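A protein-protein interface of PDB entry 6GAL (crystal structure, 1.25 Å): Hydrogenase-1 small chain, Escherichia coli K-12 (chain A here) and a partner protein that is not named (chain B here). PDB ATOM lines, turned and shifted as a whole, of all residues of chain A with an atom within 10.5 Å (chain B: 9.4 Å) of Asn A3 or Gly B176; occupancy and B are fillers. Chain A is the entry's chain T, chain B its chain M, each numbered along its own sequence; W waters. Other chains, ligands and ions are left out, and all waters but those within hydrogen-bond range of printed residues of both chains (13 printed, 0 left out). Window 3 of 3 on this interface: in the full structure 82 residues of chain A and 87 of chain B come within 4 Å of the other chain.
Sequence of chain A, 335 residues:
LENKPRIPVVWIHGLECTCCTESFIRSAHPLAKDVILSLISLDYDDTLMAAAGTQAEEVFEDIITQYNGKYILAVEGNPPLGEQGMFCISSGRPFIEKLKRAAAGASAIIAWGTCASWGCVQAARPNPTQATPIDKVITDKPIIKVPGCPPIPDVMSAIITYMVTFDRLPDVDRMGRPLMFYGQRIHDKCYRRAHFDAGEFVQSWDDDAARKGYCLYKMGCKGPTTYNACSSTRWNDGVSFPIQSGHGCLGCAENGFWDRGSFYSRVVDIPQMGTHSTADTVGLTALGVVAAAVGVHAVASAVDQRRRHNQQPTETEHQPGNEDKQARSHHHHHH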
ATOM      1  N   GLU A   2      15.646   3.114 -22.417  1.00  0.00           N
ATOM      2  CA  GLU A   2      16.116   2.105 -21.425  1.00  0.00           C
ATOM      3  C   GLU A   2      17.321   2.711 -20.727  1.00  0.00           C
ATOM      4  O   GLU A   2      18.304   3.064 -21.366  1.00  0.00           O
ATOM      5  CB  GLU A   2      16.505   0.759 -22.062  1.00  0.00           C
ATOM      6  N   ASN A   3      17.221   2.940 -19.425  1.00  0.00           N
ATOM      7  CA  ASN A   3      18.429   3.361 -18.705  1.00  0.00           C
ATOM      8  C   ASN A   3      19.217   2.093 -18.480  1.00  0.00           C
ATOM      9  O   ASN A   3      18.688   1.160 -17.829  1.00  0.00           O
ATOM     10  CB  ASN A   3      18.140   4.005 -17.375  1.00  0.00           C
ATOM     11  CG  ASN A   3      19.331   4.810 -16.893  1.00  0.00           C
ATOM     12  OD1 ASN A   3      20.454   4.316 -16.823  1.00  0.00           O
ATOM     13  ND2 ASN A   3      19.100   6.080 -16.634  1.00  0.00           N
ATOM     14  N   LYS A   4      20.432   2.058 -19.049  1.00  0.00           N
ATOM     15  CA  LYS A   4      21.281   0.851 -19.064  1.00  0.00           C
ATOM     16  C   LYS A   4      22.544   1.027 -18.200  1.00  0.00           C
ATOM     17  O   LYS A   4      23.302   1.981 -18.403  1.00  0.00           O
ATOM     18  CB  LYS A   4      21.734   0.552 -20.496  1.00  0.00           C
ATOM     19  CG  LYS A   4      22.406  -0.802 -20.650  1.00  0.00           C
ATOM     20  CD  LYS A   4      22.642  -1.193 -22.116  1.00  0.00           C
ATOM     21  CE  LYS A   4      23.870  -2.094 -22.277  1.00  0.00           C
ATOM     22  NZ  LYS A   4      23.925  -2.764 -23.609  1.00  0.00           N
ATOM     23  N   PRO A   5      22.812   0.081 -17.282  1.00  0.00           N
ATOM     24  CA  PRO A   5      23.962   0.281 -16.400  1.00  0.00           C
ATOM     25  C   PRO A   5      25.305   0.198 -17.132  1.00  0.00           C
ATOM     26  O   PRO A   5      25.419  -0.418 -18.193  1.00  0.00           O
ATOM     27  CB  PRO A   5      23.865  -0.857 -15.383  1.00  0.00           C
ATOM     28  CG  PRO A   5      22.790  -1.756 -15.829  1.00  0.00           C
ATOM     29  CD  PRO A   5      22.033  -1.125 -16.950  1.00  0.00           C
ATOM     30  N   ARG A   6      26.307   0.784 -16.507  1.00  0.00           N
ATOM     31  CA  ARG A   6      27.683   0.798 -16.989  1.00  0.00           C
ATOM     32  C   ARG A   6      28.549  -0.087 -16.092  1.00  0.00           C
ATOM     33  O   ARG A   6      28.186  -0.346 -14.923  1.00  0.00           O
ATOM     34  CB  ARG A   6      28.206   2.223 -17.029  1.00  0.00           C
ATOM     35  CG  ARG A   6      27.638   3.017 -18.204  1.00  0.00           C
ATOM     36  CD  ARG A   6      27.574   4.528 -18.012  1.00  0.00           C
ATOM     37  NE  ARG A   6      26.529   4.945 -17.077  1.00  0.00           N
ATOM     38  CZ  ARG A   6      26.746   5.584 -15.932  1.00  0.00           C
ATOM     39  NH1 ARG A   6      27.982   5.904 -15.554  1.00  0.00           N
ATOM     40  NH2 ARG A   6      25.718   5.907 -15.151  1.00  0.00           N
ATOM     41  N   ILE A   7      29.686  -0.543 -16.615  1.00  0.00           N
ATOM     42  CA  ILE A   7      30.575  -1.400 -15.868  1.00  0.00           C
ATOM     43  C   ILE A   7      31.124  -0.679 -14.627  1.00  0.00           C
ATOM     44  O   ILE A   7      31.643   0.418 -14.740  1.00  0.00           O
ATOM     45  CB  ILE A   7      31.720  -1.927 -16.737  1.00  0.00           C
ATOM     46  CG1 ILE A   7      32.571  -2.931 -15.955  1.00  0.00           C
ATOM     47  CG2 ILE A   7      32.604  -0.803 -17.278  1.00  0.00           C
ATOM     48  CD1 ILE A   7      33.455  -3.741 -16.903  1.00  0.00           C
ATOM     49  N   LEU A  37      30.630   9.794 -17.476  1.00  0.00           N
ATOM     50  CA  LEU A  37      29.186   9.959 -17.601  1.00  0.00           C
ATOM     51  C   LEU A  37      28.544   8.822 -18.450  1.00  0.00           C
ATOM     52  O   LEU A  37      27.400   8.437 -18.177  1.00  0.00           O
ATOM     53  CB  LEU A  37      28.806  11.390 -18.037  1.00  0.00           C
ATOM     54  CG  LEU A  37      29.142  12.531 -16.998  1.00  0.00           C
ATOM     55  CD1 LEU A  37      28.762  13.874 -17.619  1.00  0.00           C
ATOM     56  CD2 LEU A  37      28.551  12.399 -15.562  1.00  0.00           C
ATOM     57  N   SER A  38      29.293   8.261 -19.412  1.00  0.00           N
ATOM     58  CA  SER A  38      28.683   7.422 -20.451  1.00  0.00           C
ATOM     59  C   SER A  38      29.305   6.060 -20.679  1.00  0.00           C
ATOM     60  O   SER A  38      28.652   5.180 -21.218  1.00  0.00           O
ATOM     61  CB  SER A  38      28.612   8.198 -21.796  1.00  0.00           C
ATOM     62  OG  SER A  38      27.762   9.338 -21.674  1.00  0.00           O
ATOM     63  N   ILE A  40      31.771   4.155 -18.355  1.00  0.00           N
ATOM     64  CA  ILE A  40      31.993   3.349 -17.156  1.00  0.00           C
ATOM     65  C   ILE A  40      31.126   3.956 -16.044  1.00  0.00           C
ATOM     66  O   ILE A  40      30.614   5.062 -16.176  1.00  0.00           O
ATOM     67  CB  ILE A  40      33.501   3.285 -16.716  1.00  0.00           C
ATOM     68  CG1 ILE A  40      34.007   4.674 -16.227  1.00  0.00           C
ATOM     69  CG2 ILE A  40      34.319   2.732 -17.865  1.00  0.00           C
ATOM     70  CD1 ILE A  40      35.405   4.699 -15.668  1.00  0.00           C
ATOM     71  N   SER A  41      31.068   3.222 -14.929  1.00  0.00           N
ATOM     72  CA  SER A  41      30.554   3.791 -13.708  1.00  0.00           C
ATOM     73  C   SER A  41      31.726   3.903 -12.738  1.00  0.00           C
ATOM     74  O   SER A  41      32.173   2.894 -12.179  1.00  0.00           O
ATOM     75  CB  SER A  41      29.435   2.946 -13.095  1.00  0.00           C
ATOM     76  OG  SER A  41      28.809   3.606 -12.016  1.00  0.00           O
ATOM     77  N   ASP A  43      32.921   4.349  -9.612  1.00  0.00           N
ATOM     78  CA  ASP A  43      32.169   4.192  -8.384  1.00  0.00           C
ATOM     79  C   ASP A  43      32.919   4.493  -7.095  1.00  0.00           C
ATOM     80  O   ASP A  43      32.306   4.641  -6.060  1.00  0.00           O
ATOM     81  CB  ASP A  43      31.633   2.753  -8.291  1.00  0.00           C
ATOM     82  CG  ASP A  43      30.561   2.449  -9.318  1.00  0.00           C
ATOM     83  OD1 ASP A  43      29.854   3.409  -9.730  1.00  0.00           O
ATOM     84  OD2 ASP A  43      30.410   1.254  -9.670  1.00  0.00           O
ATOM     85  N   GLN A  66      27.959  -5.250  -3.442  1.00  0.00           N
ATOM     86  CA  GLN A  66      26.883  -5.365  -4.428  1.00  0.00           C
ATOM     87  C   GLN A  66      27.392  -5.876  -5.768  1.00  0.00           C
ATOM     88  O   GLN A  66      26.767  -6.734  -6.393  1.00  0.00           O
ATOM     89  CB  GLN A  66      26.128  -4.031  -4.606  1.00  0.00           C
ATOM     90  CG  GLN A  66      25.022  -4.143  -5.636  1.00  0.00           C
ATOM     91  CD  GLN A  66      24.217  -2.878  -5.766  1.00  0.00           C
ATOM     92  OE1 GLN A  66      24.338  -1.972  -4.933  1.00  0.00           O
ATOM     93  NE2 GLN A  66      23.375  -2.820  -6.768  1.00  0.00           N
ATOM     94  N   TYR A  67      28.573  -5.404  -6.168  1.00  0.00           N
ATOM     95  CA  TYR A  67      29.146  -5.724  -7.475  1.00  0.00           C
ATOM     96  C   TYR A  67      30.291  -6.721  -7.391  1.00  0.00           C
ATOM     97  O   TYR A  67      31.098  -6.828  -8.327  1.00  0.00           O
ATOM     98  CB  TYR A  67      29.535  -4.444  -8.187  1.00  0.00           C
ATOM     99  CG  TYR A  67      28.304  -3.613  -8.507  1.00  0.00           C
ATOM    100  CD1 TYR A  67      27.499  -3.928  -9.609  1.00  0.00           C
ATOM    101  CD2 TYR A  67      27.941  -2.518  -7.728  1.00  0.00           C
ATOM    102  CE1 TYR A  67      26.371  -3.202  -9.920  1.00  0.00           C
ATOM    103  CE2 TYR A  67      26.785  -1.792  -8.014  1.00  0.00           C
ATOM    104  CZ  TYR A  67      26.008  -2.125  -9.127  1.00  0.00           C
ATOM    105  OH  TYR A  67      24.874  -1.379  -9.420  1.00  0.00           O
ATOM    106  N   ASN B 168      19.414  17.570 -17.930  1.00  0.00           N
ATOM    107  CA  ASN B 168      18.808  16.316 -18.383  1.00  0.00           C
ATOM    108  C   ASN B 168      19.763  15.171 -18.365  1.00  0.00           C
ATOM    109  O   ASN B 168      19.410  14.039 -18.002  1.00  0.00           O
ATOM    110  CB  ASN B 168      18.287  16.430 -19.796  1.00  0.00           C
ATOM    111  CG  ASN B 168      16.902  16.891 -19.823  1.00  0.00           C
ATOM    112  OD1 ASN B 168      16.130  16.622 -18.900  1.00  0.00           O
ATOM    113  ND2 ASN B 168      16.546  17.579 -20.889  1.00  0.00           N
ATOM    114  N   ARG B 169      21.015  15.447 -18.738  1.00  0.00           N
ATOM    115  CA  ARG B 169      22.042  14.417 -18.653  1.00  0.00           C
ATOM    116  C   ARG B 169      22.277  14.008 -17.206  1.00  0.00           C
ATOM    117  O   ARG B 169      22.389  12.814 -16.904  1.00  0.00           O
ATOM    118  CB  ARG B 169      23.332  14.868 -19.310  1.00  0.00           C
ATOM    119  CG  ARG B 169      24.424  13.817 -19.405  1.00  0.00           C
ATOM    120  CD  ARG B 169      25.686  14.344 -20.071  1.00  0.00           C
ATOM    121  NE  ARG B 169      26.556  13.235 -20.480  1.00  0.00           N
ATOM    122  CZ  ARG B 169      27.708  13.401 -21.112  1.00  0.00           C
ATOM    123  NH1 ARG B 169      28.167  14.626 -21.431  1.00  0.00           N
ATOM    124  NH2 ARG B 169      28.413  12.333 -21.427  1.00  0.00           N
ATOM    125  N   LEU B 170      22.333  14.979 -16.309  1.00  0.00           N
ATOM    126  CA  LEU B 170      22.499  14.650 -14.894  1.00  0.00           C
ATOM    127  C   LEU B 170      21.269  13.882 -14.381  1.00  0.00           C
ATOM    128  O   LEU B 170      21.398  12.932 -13.611  1.00  0.00           O
ATOM    129  CB  LEU B 170      22.717  15.931 -14.065  1.00  0.00           C
ATOM    130  CG  LEU B 170      22.886  15.728 -12.552  1.00  0.00           C
ATOM    131  CD1 LEU B 170      24.128  14.910 -12.227  1.00  0.00           C
ATOM    132  CD2 LEU B 170      22.930  17.091 -11.861  1.00  0.00           C
ATOM    133  N   LYS B 171      20.078  14.314 -14.814  1.00  0.00           N
ATOM    134  CA  LYS B 171      18.867  13.665 -14.341  1.00  0.00           C
ATOM    135  C   LYS B 171      18.863  12.179 -14.696  1.00  0.00           C
ATOM    136  O   LYS B 171      18.545  11.355 -13.826  1.00  0.00           O
ATOM    137  CB  LYS B 171      17.663  14.384 -14.946  1.00  0.00           C
ATOM    138  CG  LYS B 171      16.302  13.857 -14.522  1.00  0.00           C
ATOM    139  CD  LYS B 171      15.238  14.490 -15.416  1.00  0.00           C
ATOM    140  CE  LYS B 171      14.138  13.524 -15.765  1.00  0.00           C
ATOM    141  NZ  LYS B 171      12.970  14.201 -16.373  1.00  0.00           N
ATOM    142  N   LYS B 172      19.250  11.843 -15.933  1.00  0.00           N
ATOM    143  CA  LYS B 172      19.238  10.480 -16.397  1.00  0.00           C
ATOM    144  C   LYS B 172      20.363   9.671 -15.751  1.00  0.00           C
ATOM    145  O   LYS B 172      20.167   8.506 -15.414  1.00  0.00           O
ATOM    146  CB  LYS B 172      19.288  10.434 -17.896  1.00  0.00           C
ATOM    147  CG  LYS B 172      17.992  10.972 -18.519  1.00  0.00           C
ATOM    148  CD  LYS B 172      17.898  10.563 -19.988  1.00  0.00           C
ATOM    149  CE  LYS B 172      17.468  11.714 -20.904  1.00  0.00           C
ATOM    150  NZ  LYS B 172      17.884  11.480 -22.320  1.00  0.00           N
ATOM    151  N   PHE B 173      21.509  10.313 -15.502  1.00  0.00           N
ATOM    152  CA  PHE B 173      22.610   9.693 -14.754  1.00  0.00           C
ATOM    153  C   PHE B 173      22.108   9.276 -13.366  1.00  0.00           C
ATOM    154  O   PHE B 173      22.282   8.136 -12.947  1.00  0.00           O
ATOM    155  CB  PHE B 173      23.782  10.696 -14.685  1.00  0.00           C
ATOM    156  CG  PHE B 173      25.022  10.168 -14.024  1.00  0.00           C
ATOM    157  CD1 PHE B 173      26.003   9.498 -14.755  1.00  0.00           C
ATOM    158  CD2 PHE B 173      25.227  10.380 -12.684  1.00  0.00           C
ATOM    159  CE1 PHE B 173      27.158   9.060 -14.126  1.00  0.00           C
ATOM    160  CE2 PHE B 173      26.363   9.956 -12.072  1.00  0.00           C
ATOM    161  CZ  PHE B 173      27.338   9.290 -12.784  1.00  0.00           C
ATOM    162  N   VAL B 174      21.495  10.209 -12.643  1.00  0.00           N
ATOM    163  CA  VAL B 174      20.968   9.912 -11.328  1.00  0.00           C
ATOM    164  C   VAL B 174      19.845   8.852 -11.364  1.00  0.00           C
ATOM    165  O   VAL B 174      19.848   7.917 -10.549  1.00  0.00           O
ATOM    166  CB  VAL B 174      20.574  11.192 -10.597  1.00  0.00           C
ATOM    167  CG1 VAL B 174      19.907  10.875  -9.255  1.00  0.00           C
ATOM    168  CG2 VAL B 174      21.792  12.097 -10.387  1.00  0.00           C
ATOM    169  N   GLU B 175      18.943   8.945 -12.346  1.00  0.00           N
ATOM    170  CA  GLU B 175      17.872   7.921 -12.486  1.00  0.00           C
ATOM    171  C   GLU B 175      18.432   6.531 -12.667  1.00  0.00           C
ATOM    172  O   GLU B 175      17.796   5.570 -12.264  1.00  0.00           O
ATOM    173  CB  GLU B 175      16.968   8.219 -13.679  1.00  0.00           C
ATOM    174  CG  GLU B 175      16.018   9.364 -13.458  1.00  0.00           C
ATOM    175  CD  GLU B 175      15.205   9.763 -14.680  1.00  0.00           C
ATOM    176  OE1 GLU B 175      14.278  10.546 -14.459  1.00  0.00           O
ATOM    177  OE2 GLU B 175      15.510   9.338 -15.829  1.00  0.00           O
ATOM    178  N   GLY B 176      19.585   6.420 -13.341  1.00  0.00           N
ATOM    179  CA  GLY B 176      20.195   5.129 -13.570  1.00  0.00           C
ATOM    180  C   GLY B 176      20.640   4.434 -12.302  1.00  0.00           C
ATOM    181  O   GLY B 176      20.837   3.248 -12.294  1.00  0.00           O
ATOM    182  N   GLY B 177      20.814   5.186 -11.220  1.00  0.00           N
ATOM    183  CA  GLY B 177      21.080   4.572  -9.925  1.00  0.00           C
ATOM    184  C   GLY B 177      22.541   4.332  -9.598  1.00  0.00           C
ATOM    185  O   GLY B 177      22.812   3.854  -8.491  1.00  0.00           O
ATOM    186  N   GLN B 178      23.458   4.610 -10.543  1.00  0.00           N
ATOM    187  CA  GLN B 178      24.913   4.506 -10.296  1.00  0.00           C
ATOM    188  C   GLN B 178      25.412   5.922 -10.162  1.00  0.00           C
ATOM    189  O   GLN B 178      25.747   6.575 -11.156  1.00  0.00           O
ATOM    190  CB  GLN B 178      25.620   3.767 -11.444  1.00  0.00           C
ATOM    191  CG  GLN B 178      25.140   2.343 -11.626  1.00  0.00           C
ATOM    192  CD  GLN B 178      25.819   1.732 -12.829  1.00  0.00           C
ATOM    193  OE1 GLN B 178      25.510   2.100 -13.991  1.00  0.00           O
ATOM    194  NE2 GLN B 178      26.759   0.838 -12.583  1.00  0.00           N
ATOM    195  N   LEU B 179      25.412   6.444  -8.940  1.00  0.00           N
ATOM    196  CA  LEU B 179      25.718   7.855  -8.707  1.00  0.00           C
ATOM    197  C   LEU B 179      27.174   8.198  -8.801  1.00  0.00           C
ATOM    198  O   LEU B 179      27.512   9.366  -8.852  1.00  0.00           O
ATOM    199  CB  LEU B 179      25.091   8.354  -7.397  1.00  0.00           C
ATOM    200  CG  LEU B 179      23.640   8.879  -7.512  1.00  0.00           C
ATOM    201  CD1 LEU B 179      22.685   7.892  -8.110  1.00  0.00           C
ATOM    202  CD2 LEU B 179      23.169   9.397  -6.142  1.00  0.00           C
ATOM    203  N   GLY B 180      28.028   7.175  -8.861  1.00  0.00           N
ATOM    204  CA  GLY B 180      29.429   7.425  -9.133  1.00  0.00           C
ATOM    205  C   GLY B 180      30.062   8.331  -8.089  1.00  0.00           C
ATOM    206  O   GLY B 180      29.895   8.138  -6.874  1.00  0.00           O
ATOM    207  N   ARG B 183      27.927   9.658  -5.196  1.00  0.00           N
ATOM    208  CA  ARG B 183      27.229   8.752  -4.271  1.00  0.00           C
ATOM    209  C   ARG B 183      27.574   9.055  -2.815  1.00  0.00           C
ATOM    210  O   ARG B 183      28.744   9.190  -2.429  1.00  0.00           O
ATOM    211  CB  ARG B 183      27.565   7.304  -4.606  1.00  0.00           C
ATOM    212  CG  ARG B 183      26.807   6.306  -3.752  1.00  0.00           C
ATOM    213  CD  ARG B 183      27.115   4.880  -4.154  1.00  0.00           C
ATOM    214  NE  ARG B 183      26.506   3.952  -3.201  1.00  0.00           N
ATOM    215  CZ  ARG B 183      25.754   2.895  -3.510  1.00  0.00           C
ATOM    216  NH1 ARG B 183      25.433   2.596  -4.746  1.00  0.00           N
ATOM    217  NH2 ARG B 183      25.359   2.082  -2.541  1.00  0.00           N
HETATM  218  O   HOH W   1      29.679   5.410  -6.199  1.00  0.00           O
HETATM  219  O   HOH W   2      23.860   6.055 -13.191  1.00  0.00           O
HETATM  220  O   HOH W   3      27.979   4.389  -8.099  1.00  0.00           O
HETATM  221  O   HOH W   4      24.160   0.715  -8.103  1.00  0.00           O
HETATM  222  O   HOH W   5      25.586  10.566 -19.444  1.00  0.00           O
HETATM  223  O   HOH W   6      23.340   3.490 -14.470  1.00  0.00           O
HETATM  224  O   HOH W   7      28.973  10.806 -23.412  1.00  0.00           O
HETATM  225  O   HOH W   8      23.537   0.460  -5.397  1.00  0.00           O
HETATM  226  O   HOH W   9      28.138   6.121 -12.615  1.00  0.00           O
HETATM  227  O   HOH W  10      24.676  -0.870  -2.489  1.00  0.00           O
HETATM  228  O   HOH W  11      21.069   2.063 -15.236  1.00  0.00           O
HETATM  229  O   HOH W  12      27.897   0.488  -9.943  1.00  0.00           O
HETATM  230  O   HOH W  13      26.498  -2.383 -13.744  1.00  0.00           O
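Printed residues of chain B that touch a printed residue of chain A: Arg B169, Lys B172, Phe B173, Gly B176 and Gln B178. Hydrophobic or aromatic side chains of chain B that line the printed part of chain A: Phe B173. Of the 13 printed residues of chain A, 6 touch a printed residue of chain B. Printed residues of chain A that touch a printed residue of chain B: Asn A3, Pro A5, Arg A6, Leu A37, Ser A38 and Ser A41. Hydrophobic or aromatic side chains of chain A within 4 Å of the printed part of chain B: Pro A5 and Leu A37.
Water W7 bridges NH2 of Arg B169 (2.6 Å) and OG of Ser A38 (2.6 Å). Water W8 bridges OE1 of Gln A66 (2.6 Å) and NH1 of Arg B183 (2.9 Å). Water W6 lies within hydrogen-bond range of OE1 of Gln B178 (2.6 Å), O of Gly B176 (3.3 Å) and NH2 of Arg A6 (3.5 Å). Water W11 lies within hydrogen-bond range of OD1 of Asn A3 and O of Gly B176. Water W13 lies within hydrogen-bond range of O of Arg A6 and NE2 of Gln B178. Water W5 lies within hydrogen-bond range of NE of Arg B169, O of Leu A37 and OG of Ser A38.
The backbone carbonyl oxygen (O) of Ile A7 lies within hydrogen-bond range of the backbone NH (N) of Ser A41, 2.9 Å away. The backbone carbonyl oxygen of Ile A40 is in hydrogen-bond range of the guanidinium group of Arg A6 (2.8 Å). The side-chain hydroxyl of Ser A41 is in hydrogen-bond range of the side-chain carboxylate of Asp A43 (2.5 Å).
N of Arg A6 lies within hydrogen-bond range of OE1 of Gln B178. The backbone carbonyl oxygen (O) of Lys B172 is in hydrogen-bond range of the side-chain amide nitrogen (ND2) of Asn A3 (2.9 Å). The side-chain amide nitrogen (NE2) of Gln B178 lies close to the side-chain hydroxyl (OG) of Ser A41, 3.5 Å away. The side-chain amide nitrogen (ND2) of Asn A3 lies close to the backbone NH (N) of Gly B176, at 3.3 Å. NH2 of Arg B169 is in hydrogen-bond range of OG of Ser A38, 3.1 Å away.
Of chain B, only Lys B172 (2.9 Å) and Gly B176 (3.3 Å) come within 4 Å of Asn A3. Of the printed residues of chain A, Gly B176 touches Asn A3. No residue of chain B comes within 4 Å of Glu A2. No residue of chain A comes within 4 Å of Gly B177. Printed residues of chain A within 4 Å of Lys B172: Asn A3 (2.9 Å). Of the printed residues of chain A, Gln B178 touches Pro A5, Arg A6 and Ser A41. Printed residues of chain B within 4 Å of Ser A41: Gln B178 (3.2 Å). Asn B168 touches none of the printed residues of chain A. The nearest printed residue of chain A that does not touch Gly B176 is Arg A6 (5.8 Å).
OE1 of Gln B178 touches CA of Pro A5, 3.4 Å away. CE1 of Phe B173 touches NH1 of Arg A6, 3.6 Å away. Arg B169 touches Leu A37. Phe B173 touches Leu A37 (CD1 to O, 3.8 Å).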
